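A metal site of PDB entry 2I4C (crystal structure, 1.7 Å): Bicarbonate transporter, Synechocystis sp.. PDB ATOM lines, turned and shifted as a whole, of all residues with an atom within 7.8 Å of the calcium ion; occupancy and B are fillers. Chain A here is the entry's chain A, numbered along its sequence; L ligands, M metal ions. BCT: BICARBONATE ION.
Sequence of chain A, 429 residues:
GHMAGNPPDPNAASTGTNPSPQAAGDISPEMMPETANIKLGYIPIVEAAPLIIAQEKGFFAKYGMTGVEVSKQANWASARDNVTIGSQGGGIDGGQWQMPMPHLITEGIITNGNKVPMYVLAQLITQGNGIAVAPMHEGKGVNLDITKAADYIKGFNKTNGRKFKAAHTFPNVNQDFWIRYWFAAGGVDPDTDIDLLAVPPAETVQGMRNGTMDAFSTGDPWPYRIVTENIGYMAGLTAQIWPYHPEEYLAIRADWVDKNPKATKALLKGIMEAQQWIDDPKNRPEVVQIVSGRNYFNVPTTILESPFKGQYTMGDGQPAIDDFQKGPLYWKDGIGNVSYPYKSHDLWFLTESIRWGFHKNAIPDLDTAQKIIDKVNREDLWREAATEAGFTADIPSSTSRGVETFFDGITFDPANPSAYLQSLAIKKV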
ATOM      1  N   ILE A  45      -9.335  -0.054 -13.294  1.00  0.00           N
ATOM      2  CA  ILE A  45     -10.190  -0.968 -12.537  1.00  0.00           C
ATOM      3  C   ILE A  45     -11.055  -0.110 -11.610  1.00  0.00           C
ATOM      4  O   ILE A  45     -10.711   1.035 -11.327  1.00  0.00           O
ATOM      5  CB  ILE A  45      -9.364  -1.982 -11.733  1.00  0.00           C
ATOM      6  CG1 ILE A  45      -8.266  -1.259 -10.944  1.00  0.00           C
ATOM      7  CG2 ILE A  45      -8.763  -3.028 -12.677  1.00  0.00           C
ATOM      8  CD1 ILE A  45      -7.399  -2.190 -10.130  1.00  0.00           C
ATOM      9  N   VAL A  46     -12.162  -0.662 -11.128  1.00  0.00           N
ATOM     10  CA  VAL A  46     -13.063   0.118 -10.279  1.00  0.00           C
ATOM     11  C   VAL A  46     -12.416   0.822  -9.086  1.00  0.00           C
ATOM     12  O   VAL A  46     -12.952   1.808  -8.590  1.00  0.00           O
ATOM     13  CB  VAL A  46     -14.248  -0.732  -9.766  1.00  0.00           C
ATOM     14  CG1 VAL A  46     -15.069  -1.222 -10.951  1.00  0.00           C
ATOM     15  CG2 VAL A  46     -13.746  -1.905  -8.922  1.00  0.00           C
ATOM     16  N   GLU A  47     -11.266   0.319  -8.630  1.00  0.00           N
ATOM     17  CA  GLU A  47     -10.565   0.922  -7.506  1.00  0.00           C
ATOM     18  C   GLU A  47     -10.155   2.362  -7.792  1.00  0.00           C
ATOM     19  O   GLU A  47      -9.951   3.162  -6.871  1.00  0.00           O
ATOM     20  CB  GLU A  47      -9.301   0.114  -7.143  1.00  0.00           C
ATOM     21  CG  GLU A  47      -9.594  -1.260  -6.549  1.00  0.00           C
ATOM     22  CD  GLU A  47      -9.737  -2.352  -7.595  1.00  0.00           C
ATOM     23  OE1 GLU A  47     -10.331  -2.090  -8.667  1.00  0.00           O
ATOM     24  OE2 GLU A  47      -9.276  -3.477  -7.329  1.00  0.00           O
ATOM     25  N   TRP A  76       1.101  -2.439 -12.955  1.00  0.00           N
ATOM     26  CA  TRP A  76       1.598  -2.140 -11.628  1.00  0.00           C
ATOM     27  C   TRP A  76       3.096  -1.881 -11.574  1.00  0.00           C
ATOM     28  O   TRP A  76       3.547  -1.027 -10.815  1.00  0.00           O
ATOM     29  CB  TRP A  76       1.188  -3.250 -10.671  1.00  0.00           C
ATOM     30  CG  TRP A  76      -0.266  -3.150 -10.347  1.00  0.00           C
ATOM     31  CD1 TRP A  76      -1.246  -4.057 -10.623  1.00  0.00           C
ATOM     32  CD2 TRP A  76      -0.901  -2.048  -9.702  1.00  0.00           C
ATOM     33  NE1 TRP A  76      -2.467  -3.589 -10.187  1.00  0.00           N
ATOM     34  CE2 TRP A  76      -2.284  -2.360  -9.609  1.00  0.00           C
ATOM     35  CE3 TRP A  76      -0.452  -0.825  -9.191  1.00  0.00           C
ATOM     36  CZ2 TRP A  76      -3.209  -1.478  -9.031  1.00  0.00           C
ATOM     37  CZ3 TRP A  76      -1.374   0.040  -8.609  1.00  0.00           C
ATOM     38  CH2 TRP A  76      -2.736  -0.291  -8.535  1.00  0.00           C
ATOM     39  N   GLN A  96      -3.078   5.542  -7.137  1.00  0.00           N
ATOM     40  CA  GLN A  96      -3.768   4.349  -6.677  1.00  0.00           C
ATOM     41  C   GLN A  96      -2.778   3.207  -6.495  1.00  0.00           C
ATOM     42  O   GLN A  96      -1.933   2.985  -7.360  1.00  0.00           O
ATOM     43  CB  GLN A  96      -4.797   3.982  -7.742  1.00  0.00           C
ATOM     44  CG  GLN A  96      -5.513   2.660  -7.567  1.00  0.00           C
ATOM     45  CD  GLN A  96      -6.106   2.228  -8.891  1.00  0.00           C
ATOM     46  OE1 GLN A  96      -6.306   3.045  -9.788  1.00  0.00           O
ATOM     47  NE2 GLN A  96      -6.400   0.933  -9.028  1.00  0.00           N
ATOM     48  N   TRP A  97      -2.885   2.477  -5.387  1.00  0.00           N
ATOM     49  CA  TRP A  97      -1.979   1.372  -5.131  1.00  0.00           C
ATOM     50  C   TRP A  97      -2.565   0.160  -4.458  1.00  0.00           C
ATOM     51  O   TRP A  97      -3.504   0.273  -3.682  1.00  0.00           O
ATOM     52  CB  TRP A  97      -0.825   1.818  -4.233  1.00  0.00           C
ATOM     53  CG  TRP A  97      -0.155   3.042  -4.703  1.00  0.00           C
ATOM     54  CD1 TRP A  97      -0.437   4.316  -4.327  1.00  0.00           C
ATOM     55  CD2 TRP A  97       0.856   3.116  -5.710  1.00  0.00           C
ATOM     56  NE1 TRP A  97       0.337   5.194  -5.050  1.00  0.00           N
ATOM     57  CE2 TRP A  97       1.137   4.485  -5.905  1.00  0.00           C
ATOM     58  CE3 TRP A  97       1.534   2.161  -6.469  1.00  0.00           C
ATOM     59  CZ2 TRP A  97       2.075   4.919  -6.841  1.00  0.00           C
ATOM     60  CZ3 TRP A  97       2.472   2.595  -7.405  1.00  0.00           C
ATOM     61  CH2 TRP A  97       2.736   3.967  -7.577  1.00  0.00           C
ATOM     62  N   GLN A  98      -1.973  -0.990  -4.756  1.00  0.00           N
ATOM     63  CA  GLN A  98      -2.339  -2.214  -4.079  1.00  0.00           C
ATOM     64  C   GLN A  98      -1.407  -2.157  -2.882  1.00  0.00           C
ATOM     65  O   GLN A  98      -0.314  -1.602  -2.976  1.00  0.00           O
ATOM     66  CB  GLN A  98      -1.983  -3.445  -4.912  1.00  0.00           C
ATOM     67  CG  GLN A  98      -2.958  -3.743  -6.026  1.00  0.00           C
ATOM     68  CD  GLN A  98      -2.625  -5.047  -6.715  1.00  0.00           C
ATOM     69  OE1 GLN A  98      -1.900  -5.068  -7.716  1.00  0.00           O
ATOM     70  NE2 GLN A  98      -3.125  -6.139  -6.174  1.00  0.00           N
ATOM     71  N   MET A  99      -1.824  -2.728  -1.760  1.00  0.00           N
ATOM     72  CA  MET A  99      -1.016  -2.707  -0.544  1.00  0.00           C
ATOM     73  C   MET A  99      -0.134  -3.942  -0.491  1.00  0.00           C
ATOM     74  O   MET A  99      -0.524  -5.007  -0.979  1.00  0.00           O
ATOM     75  CB  MET A  99      -1.928  -2.661   0.670  1.00  0.00           C
ATOM     76  CG  MET A  99      -2.735  -1.384   0.780  1.00  0.00           C
ATOM     77  SD  MET A  99      -1.711   0.014   1.248  1.00  0.00           S
ATOM     78  CE  MET A  99      -2.052   0.079   3.033  1.00  0.00           C
ATOM     79  N   ILE A 125     -11.275   2.157  -1.831  1.00  0.00           N
ATOM     80  CA  ILE A 125     -12.435   1.312  -2.001  1.00  0.00           C
ATOM     81  C   ILE A 125     -12.265  -0.003  -1.267  1.00  0.00           C
ATOM     82  O   ILE A 125     -11.176  -0.324  -0.776  1.00  0.00           O
ATOM     83  CB  ILE A 125     -12.539   1.001  -3.522  1.00  0.00           C
ATOM     84  CG1 ILE A 125     -13.725   0.090  -3.844  1.00  0.00           C
ATOM     85  CG2 ILE A 125     -11.221   0.345  -3.973  1.00  0.00           C
ATOM     86  CD1 ILE A 125     -13.741  -0.353  -5.307  1.00  0.00           C
ATOM     87  N   GLN A 127     -13.705  -4.235  -1.693  1.00  0.00           N
ATOM     88  CA  GLN A 127     -14.348  -5.191  -2.598  1.00  0.00           C
ATOM     89  C   GLN A 127     -14.201  -4.813  -4.068  1.00  0.00           C
ATOM     90  O   GLN A 127     -13.295  -4.065  -4.436  1.00  0.00           O
ATOM     91  CB  GLN A 127     -15.820  -5.355  -2.186  1.00  0.00           C
ATOM     92  CG  GLN A 127     -15.912  -5.524  -0.679  1.00  0.00           C
ATOM     93  CD  GLN A 127     -17.301  -5.807  -0.161  1.00  0.00           C
ATOM     94  OE1 GLN A 127     -18.291  -5.291  -0.677  1.00  0.00           O
ATOM     95  NE2 GLN A 127     -17.363  -6.599   0.892  1.00  0.00           N
ATOM     96  N   GLY A 128     -15.080  -5.347  -4.918  1.00  0.00           N
ATOM     97  CA  GLY A 128     -14.968  -5.059  -6.339  1.00  0.00           C
ATOM     98  C   GLY A 128     -13.884  -5.930  -6.942  1.00  0.00           C
ATOM     99  O   GLY A 128     -13.418  -5.704  -8.065  1.00  0.00           O
ATOM    100  N   ASN A 129     -13.488  -6.947  -6.190  1.00  0.00           N
ATOM    101  CA  ASN A 129     -12.459  -7.892  -6.610  1.00  0.00           C
ATOM    102  C   ASN A 129     -12.947  -9.321  -6.489  1.00  0.00           C
ATOM    103  O   ASN A 129     -13.872  -9.615  -5.733  1.00  0.00           O
ATOM    104  CB  ASN A 129     -11.197  -7.699  -5.773  1.00  0.00           C
ATOM    105  CG  ASN A 129     -10.418  -6.466  -6.173  1.00  0.00           C
ATOM    106  OD1 ASN A 129      -9.384  -6.563  -6.809  1.00  0.00           O
ATOM    107  ND2 ASN A 129     -10.913  -5.287  -5.798  1.00  0.00           N
ATOM    108  N   GLY A 130     -12.329 -10.235  -7.236  1.00  0.00           N
ATOM    109  CA  GLY A 130     -12.741 -11.623  -7.172  1.00  0.00           C
ATOM    110  C   GLY A 130     -11.755 -12.561  -7.838  1.00  0.00           C
ATOM    111  O   GLY A 130     -10.785 -12.137  -8.465  1.00  0.00           O
ATOM    112  N   THR A 169      -1.904  -9.764 -10.422  1.00  0.00           N
ATOM    113  CA  THR A 169      -1.442  -8.641 -11.236  1.00  0.00           C
ATOM    114  C   THR A 169      -0.124  -7.985 -10.806  1.00  0.00           C
ATOM    115  O   THR A 169       0.309  -7.008 -11.407  1.00  0.00           O
ATOM    116  CB  THR A 169      -2.503  -7.529 -11.262  1.00  0.00           C
ATOM    117  OG1 THR A 169      -2.729  -7.062  -9.921  1.00  0.00           O
ATOM    118  CG2 THR A 169      -3.813  -8.069 -11.828  1.00  0.00           C
ATOM    119  N   ASN A 174      -2.165  -7.002  -2.757  1.00  0.00           N
ATOM    120  CA  ASN A 174      -3.564  -7.411  -2.760  1.00  0.00           C
ATOM    121  C   ASN A 174      -3.951  -8.685  -3.492  1.00  0.00           C
ATOM    122  O   ASN A 174      -4.166  -9.713  -2.872  1.00  0.00           O
ATOM    123  CB  ASN A 174      -4.440  -6.261  -3.267  1.00  0.00           C
ATOM    124  CG  ASN A 174      -4.438  -5.083  -2.320  1.00  0.00           C
ATOM    125  OD1 ASN A 174      -3.393  -4.665  -1.836  1.00  0.00           O
ATOM    126  ND2 ASN A 174      -5.628  -4.533  -2.050  1.00  0.00           N
ATOM    127  N   GLN A 175      -4.052  -8.619  -4.826  1.00  0.00           N
ATOM    128  CA  GLN A 175      -4.481  -9.786  -5.603  1.00  0.00           C
ATOM    129  C   GLN A 175      -3.723 -11.074  -5.271  1.00  0.00           C
ATOM    130  O   GLN A 175      -4.307 -12.150  -5.237  1.00  0.00           O
ATOM    131  CB  GLN A 175      -4.384  -9.499  -7.106  1.00  0.00           C
ATOM    132  CG  GLN A 175      -4.991  -8.168  -7.537  1.00  0.00           C
ATOM    133  CD  GLN A 175      -6.295  -7.840  -6.833  1.00  0.00           C
ATOM    134  OE1 GLN A 175      -6.367  -6.874  -6.069  1.00  0.00           O
ATOM    135  NE2 GLN A 175      -7.321  -8.638  -7.079  1.00  0.00           N
ATOM    136  N   TRP A 178      -5.099 -12.176  -1.912  1.00  0.00           N
ATOM    137  CA  TRP A 178      -6.442 -12.713  -2.015  1.00  0.00           C
ATOM    138  C   TRP A 178      -6.452 -14.140  -2.523  1.00  0.00           C
ATOM    139  O   TRP A 178      -7.036 -15.025  -1.906  1.00  0.00           O
ATOM    140  CB  TRP A 178      -7.304 -11.842  -2.931  1.00  0.00           C
ATOM    141  CG  TRP A 178      -7.395 -10.377  -2.547  1.00  0.00           C
ATOM    142  CD1 TRP A 178      -7.603  -9.331  -3.385  1.00  0.00           C
ATOM    143  CD2 TRP A 178      -7.269  -9.822  -1.231  1.00  0.00           C
ATOM    144  NE1 TRP A 178      -7.615  -8.147  -2.688  1.00  0.00           N
ATOM    145  CE2 TRP A 178      -7.413  -8.417  -1.365  1.00  0.00           C
ATOM    146  CE3 TRP A 178      -7.044 -10.363   0.043  1.00  0.00           C
ATOM    147  CZ2 TRP A 178      -7.344  -7.544  -0.271  1.00  0.00           C
ATOM    148  CZ3 TRP A 178      -6.975  -9.490   1.137  1.00  0.00           C
ATOM    149  CH2 TRP A 178      -7.128  -8.102   0.973  1.00  0.00           C
ATOM    150  N   SER A 217      -6.620 -14.023  -9.773  1.00  0.00           N
ATOM    151  CA  SER A 217      -7.060 -13.023  -8.818  1.00  0.00           C
ATOM    152  C   SER A 217      -7.315 -11.736  -9.593  1.00  0.00           C
ATOM    153  O   SER A 217      -6.384 -11.031  -9.980  1.00  0.00           O
ATOM    154  CB  SER A 217      -5.968 -12.818  -7.763  1.00  0.00           C
ATOM    155  OG  SER A 217      -6.472 -12.128  -6.633  1.00  0.00           O
ATOM    156  N   THR A 218      -8.586 -11.434  -9.800  1.00  0.00           N
ATOM    157  CA  THR A 218      -8.947 -10.243 -10.542  1.00  0.00           C
ATOM    158  C   THR A 218      -9.948  -9.358  -9.817  1.00  0.00           C
ATOM    159  O   THR A 218     -10.215  -9.521  -8.627  1.00  0.00           O
ATOM    160  CB  THR A 218      -9.526 -10.652 -11.922  1.00  0.00           C
ATOM    161  OG1 THR A 218      -9.717  -9.486 -12.738  1.00  0.00           O
ATOM    162  CG2 THR A 218     -10.846 -11.394 -11.756  1.00  0.00           C
ATOM    163  N   GLY A 219     -10.495  -8.390 -10.558  1.00  0.00           N
ATOM    164  CA  GLY A 219     -11.454  -7.473 -10.003  1.00  0.00           C
ATOM    165  C   GLY A 219     -12.188  -6.793 -11.142  1.00  0.00           C
ATOM    166  O   GLY A 219     -11.804  -6.925 -12.310  1.00  0.00           O
ATOM    167  N   ASP A 220     -13.235  -6.042 -10.814  1.00  0.00           N
ATOM    168  CA  ASP A 220     -14.023  -5.387 -11.830  1.00  0.00           C
ATOM    169  C   ASP A 220     -13.267  -4.331 -12.628  1.00  0.00           C
ATOM    170  O   ASP A 220     -12.452  -3.590 -12.079  1.00  0.00           O
ATOM    171  CB  ASP A 220     -15.277  -4.792 -11.189  1.00  0.00           C
ATOM    172  CG  ASP A 220     -16.037  -5.831 -10.396  1.00  0.00           C
ATOM    173  OD1 ASP A 220     -16.046  -7.004 -10.826  1.00  0.00           O
ATOM    174  OD2 ASP A 220     -16.631  -5.485  -9.344  1.00  0.00           O
ATOM    175  N   THR A 238     -13.876 -11.204  -3.360  1.00  0.00           N
ATOM    176  CA  THR A 238     -13.099 -10.925  -2.159  1.00  0.00           C
ATOM    177  C   THR A 238     -14.094 -10.463  -1.102  1.00  0.00           C
ATOM    178  O   THR A 238     -13.819 -10.549   0.089  1.00  0.00           O
ATOM    179  CB  THR A 238     -12.050  -9.824  -2.409  1.00  0.00           C
ATOM    180  OG1 THR A 238     -12.675  -8.676  -2.978  1.00  0.00           O
ATOM    181  CG2 THR A 238     -10.954 -10.332  -3.331  1.00  0.00           C
ATOM    182  N   HIS A 245     -13.085  -5.897   3.254  1.00  0.00           N
ATOM    183  CA  HIS A 245     -11.632  -5.948   3.426  1.00  0.00           C
ATOM    184  C   HIS A 245     -10.963  -4.695   2.889  1.00  0.00           C
ATOM    185  O   HIS A 245     -11.486  -4.034   1.997  1.00  0.00           O
ATOM    186  CB  HIS A 245     -11.072  -7.122   2.620  1.00  0.00           C
ATOM    187  CG  HIS A 245     -11.246  -6.974   1.149  1.00  0.00           C
ATOM    188  ND1 HIS A 245     -12.408  -7.321   0.479  1.00  0.00           N
ATOM    189  CD2 HIS A 245     -10.425  -6.456   0.202  1.00  0.00           C
ATOM    190  CE1 HIS A 245     -12.294  -7.017  -0.801  1.00  0.00           C
ATOM    191  NE2 HIS A 245     -11.103  -6.483  -0.996  1.00  0.00           N
ATOM    192  N   GLU A 247      -8.736  -2.606   0.576  1.00  0.00           N
ATOM    193  CA  GLU A 247      -8.363  -2.932  -0.793  1.00  0.00           C
ATOM    194  C   GLU A 247      -7.263  -2.024  -1.305  1.00  0.00           C
ATOM    195  O   GLU A 247      -6.128  -2.104  -0.833  1.00  0.00           O
ATOM    196  CB  GLU A 247      -9.599  -2.881  -1.690  1.00  0.00           C
ATOM    197  CG  GLU A 247      -9.382  -3.296  -3.144  1.00  0.00           C
ATOM    198  CD  GLU A 247      -8.553  -4.561  -3.293  1.00  0.00           C
ATOM    199  OE1 GLU A 247      -8.633  -5.450  -2.417  1.00  0.00           O
ATOM    200  OE2 GLU A 247      -7.840  -4.688  -4.315  1.00  0.00           O
ATOM    201  N   GLU A 248      -7.572  -1.150  -2.256  1.00  0.00           N
ATOM    202  CA  GLU A 248      -6.550  -0.273  -2.804  1.00  0.00           C
ATOM    203  C   GLU A 248      -6.585   1.120  -2.190  1.00  0.00           C
ATOM    204  O   GLU A 248      -7.627   1.597  -1.738  1.00  0.00           O
ATOM    205  CB  GLU A 248      -6.632  -0.270  -4.328  1.00  0.00           C
ATOM    206  CG  GLU A 248      -6.180  -1.643  -4.865  1.00  0.00           C
ATOM    207  CD  GLU A 248      -6.090  -1.743  -6.371  1.00  0.00           C
ATOM    208  OE1 GLU A 248      -5.773  -0.744  -7.034  1.00  0.00           O
ATOM    209  OE2 GLU A 248      -6.331  -2.855  -6.884  1.00  0.00           O
HETATM  210  C   BCT L   1      -5.454  -4.884  -9.174  1.00  0.00           C
HETATM  211  O1  BCT L   1      -6.633  -5.192  -8.797  1.00  0.00           O
HETATM  212  O2  BCT L   1      -4.795  -3.980  -8.550  1.00  0.00           O
HETATM  213  O3  BCT L   1      -4.897  -5.510 -10.220  1.00  0.00           O
HETATM  214 CA    CA M   1      -7.591  -4.822  -6.540  1.00  0.00          CA
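The backbone carbonyl oxygen (O) of Glu 247 is in hydrogen-bond range of the side-chain amide nitrogen (ND2) of Asn 174 (2.8 Å).
The side-chain carboxylate (OE1) of Glu 247 sits at hydrogen-bond distance from a ring nitrogen (NE2) of His 245 (3.0 Å).
The side-chain carboxylate (OE1) of Glu 248 sits at hydrogen-bond distance from the side-chain amide nitrogen (NE2) of Gln 96 (2.7 Å).
NE2 of Gln 98 sits close to N of Gln 175 (3.0 Å).
NE2 of Gln 175 lies within hydrogen-bond range of O of Thr 218, at 3.4 Å.
O of Gln 175 sits at hydrogen-bond distance from OG of Ser 217, at 2.6 Å.
The backbone carbonyl oxygen (O) of Gln 127 sits at hydrogen-bond distance from the side-chain amide nitrogen (ND2) of Asn 129 (3.0 Å).
The backbone NH of Thr 238 lies within hydrogen-bond range of the backbone carbonyl oxygen of Asn 129 (2.9 Å).
Of the 25 residues printed, 5 come within 4 Å of the calcium ion.
The nearest printed residue that does not touch the calcium ion is Ile 45 (4.5 Å).
The side-chain carboxylate (OE2) of Glu 247 binds the calcium ion (2.2 Å).
The side-chain carboxylate (OE2) of Glu 47 is bound to the calcium ion.
The calcium ion is bound by the side-chain carboxylate (OE2) of Glu 248 (2.4 Å).
OE1 of Gln 175 binds the calcium ion.
The calcium ion is bound by O1 of the ligand (2.5 Å).
The side-chain amide oxygen (OD1) of Asn 129 is bound to the calcium ion (2.5 Å).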
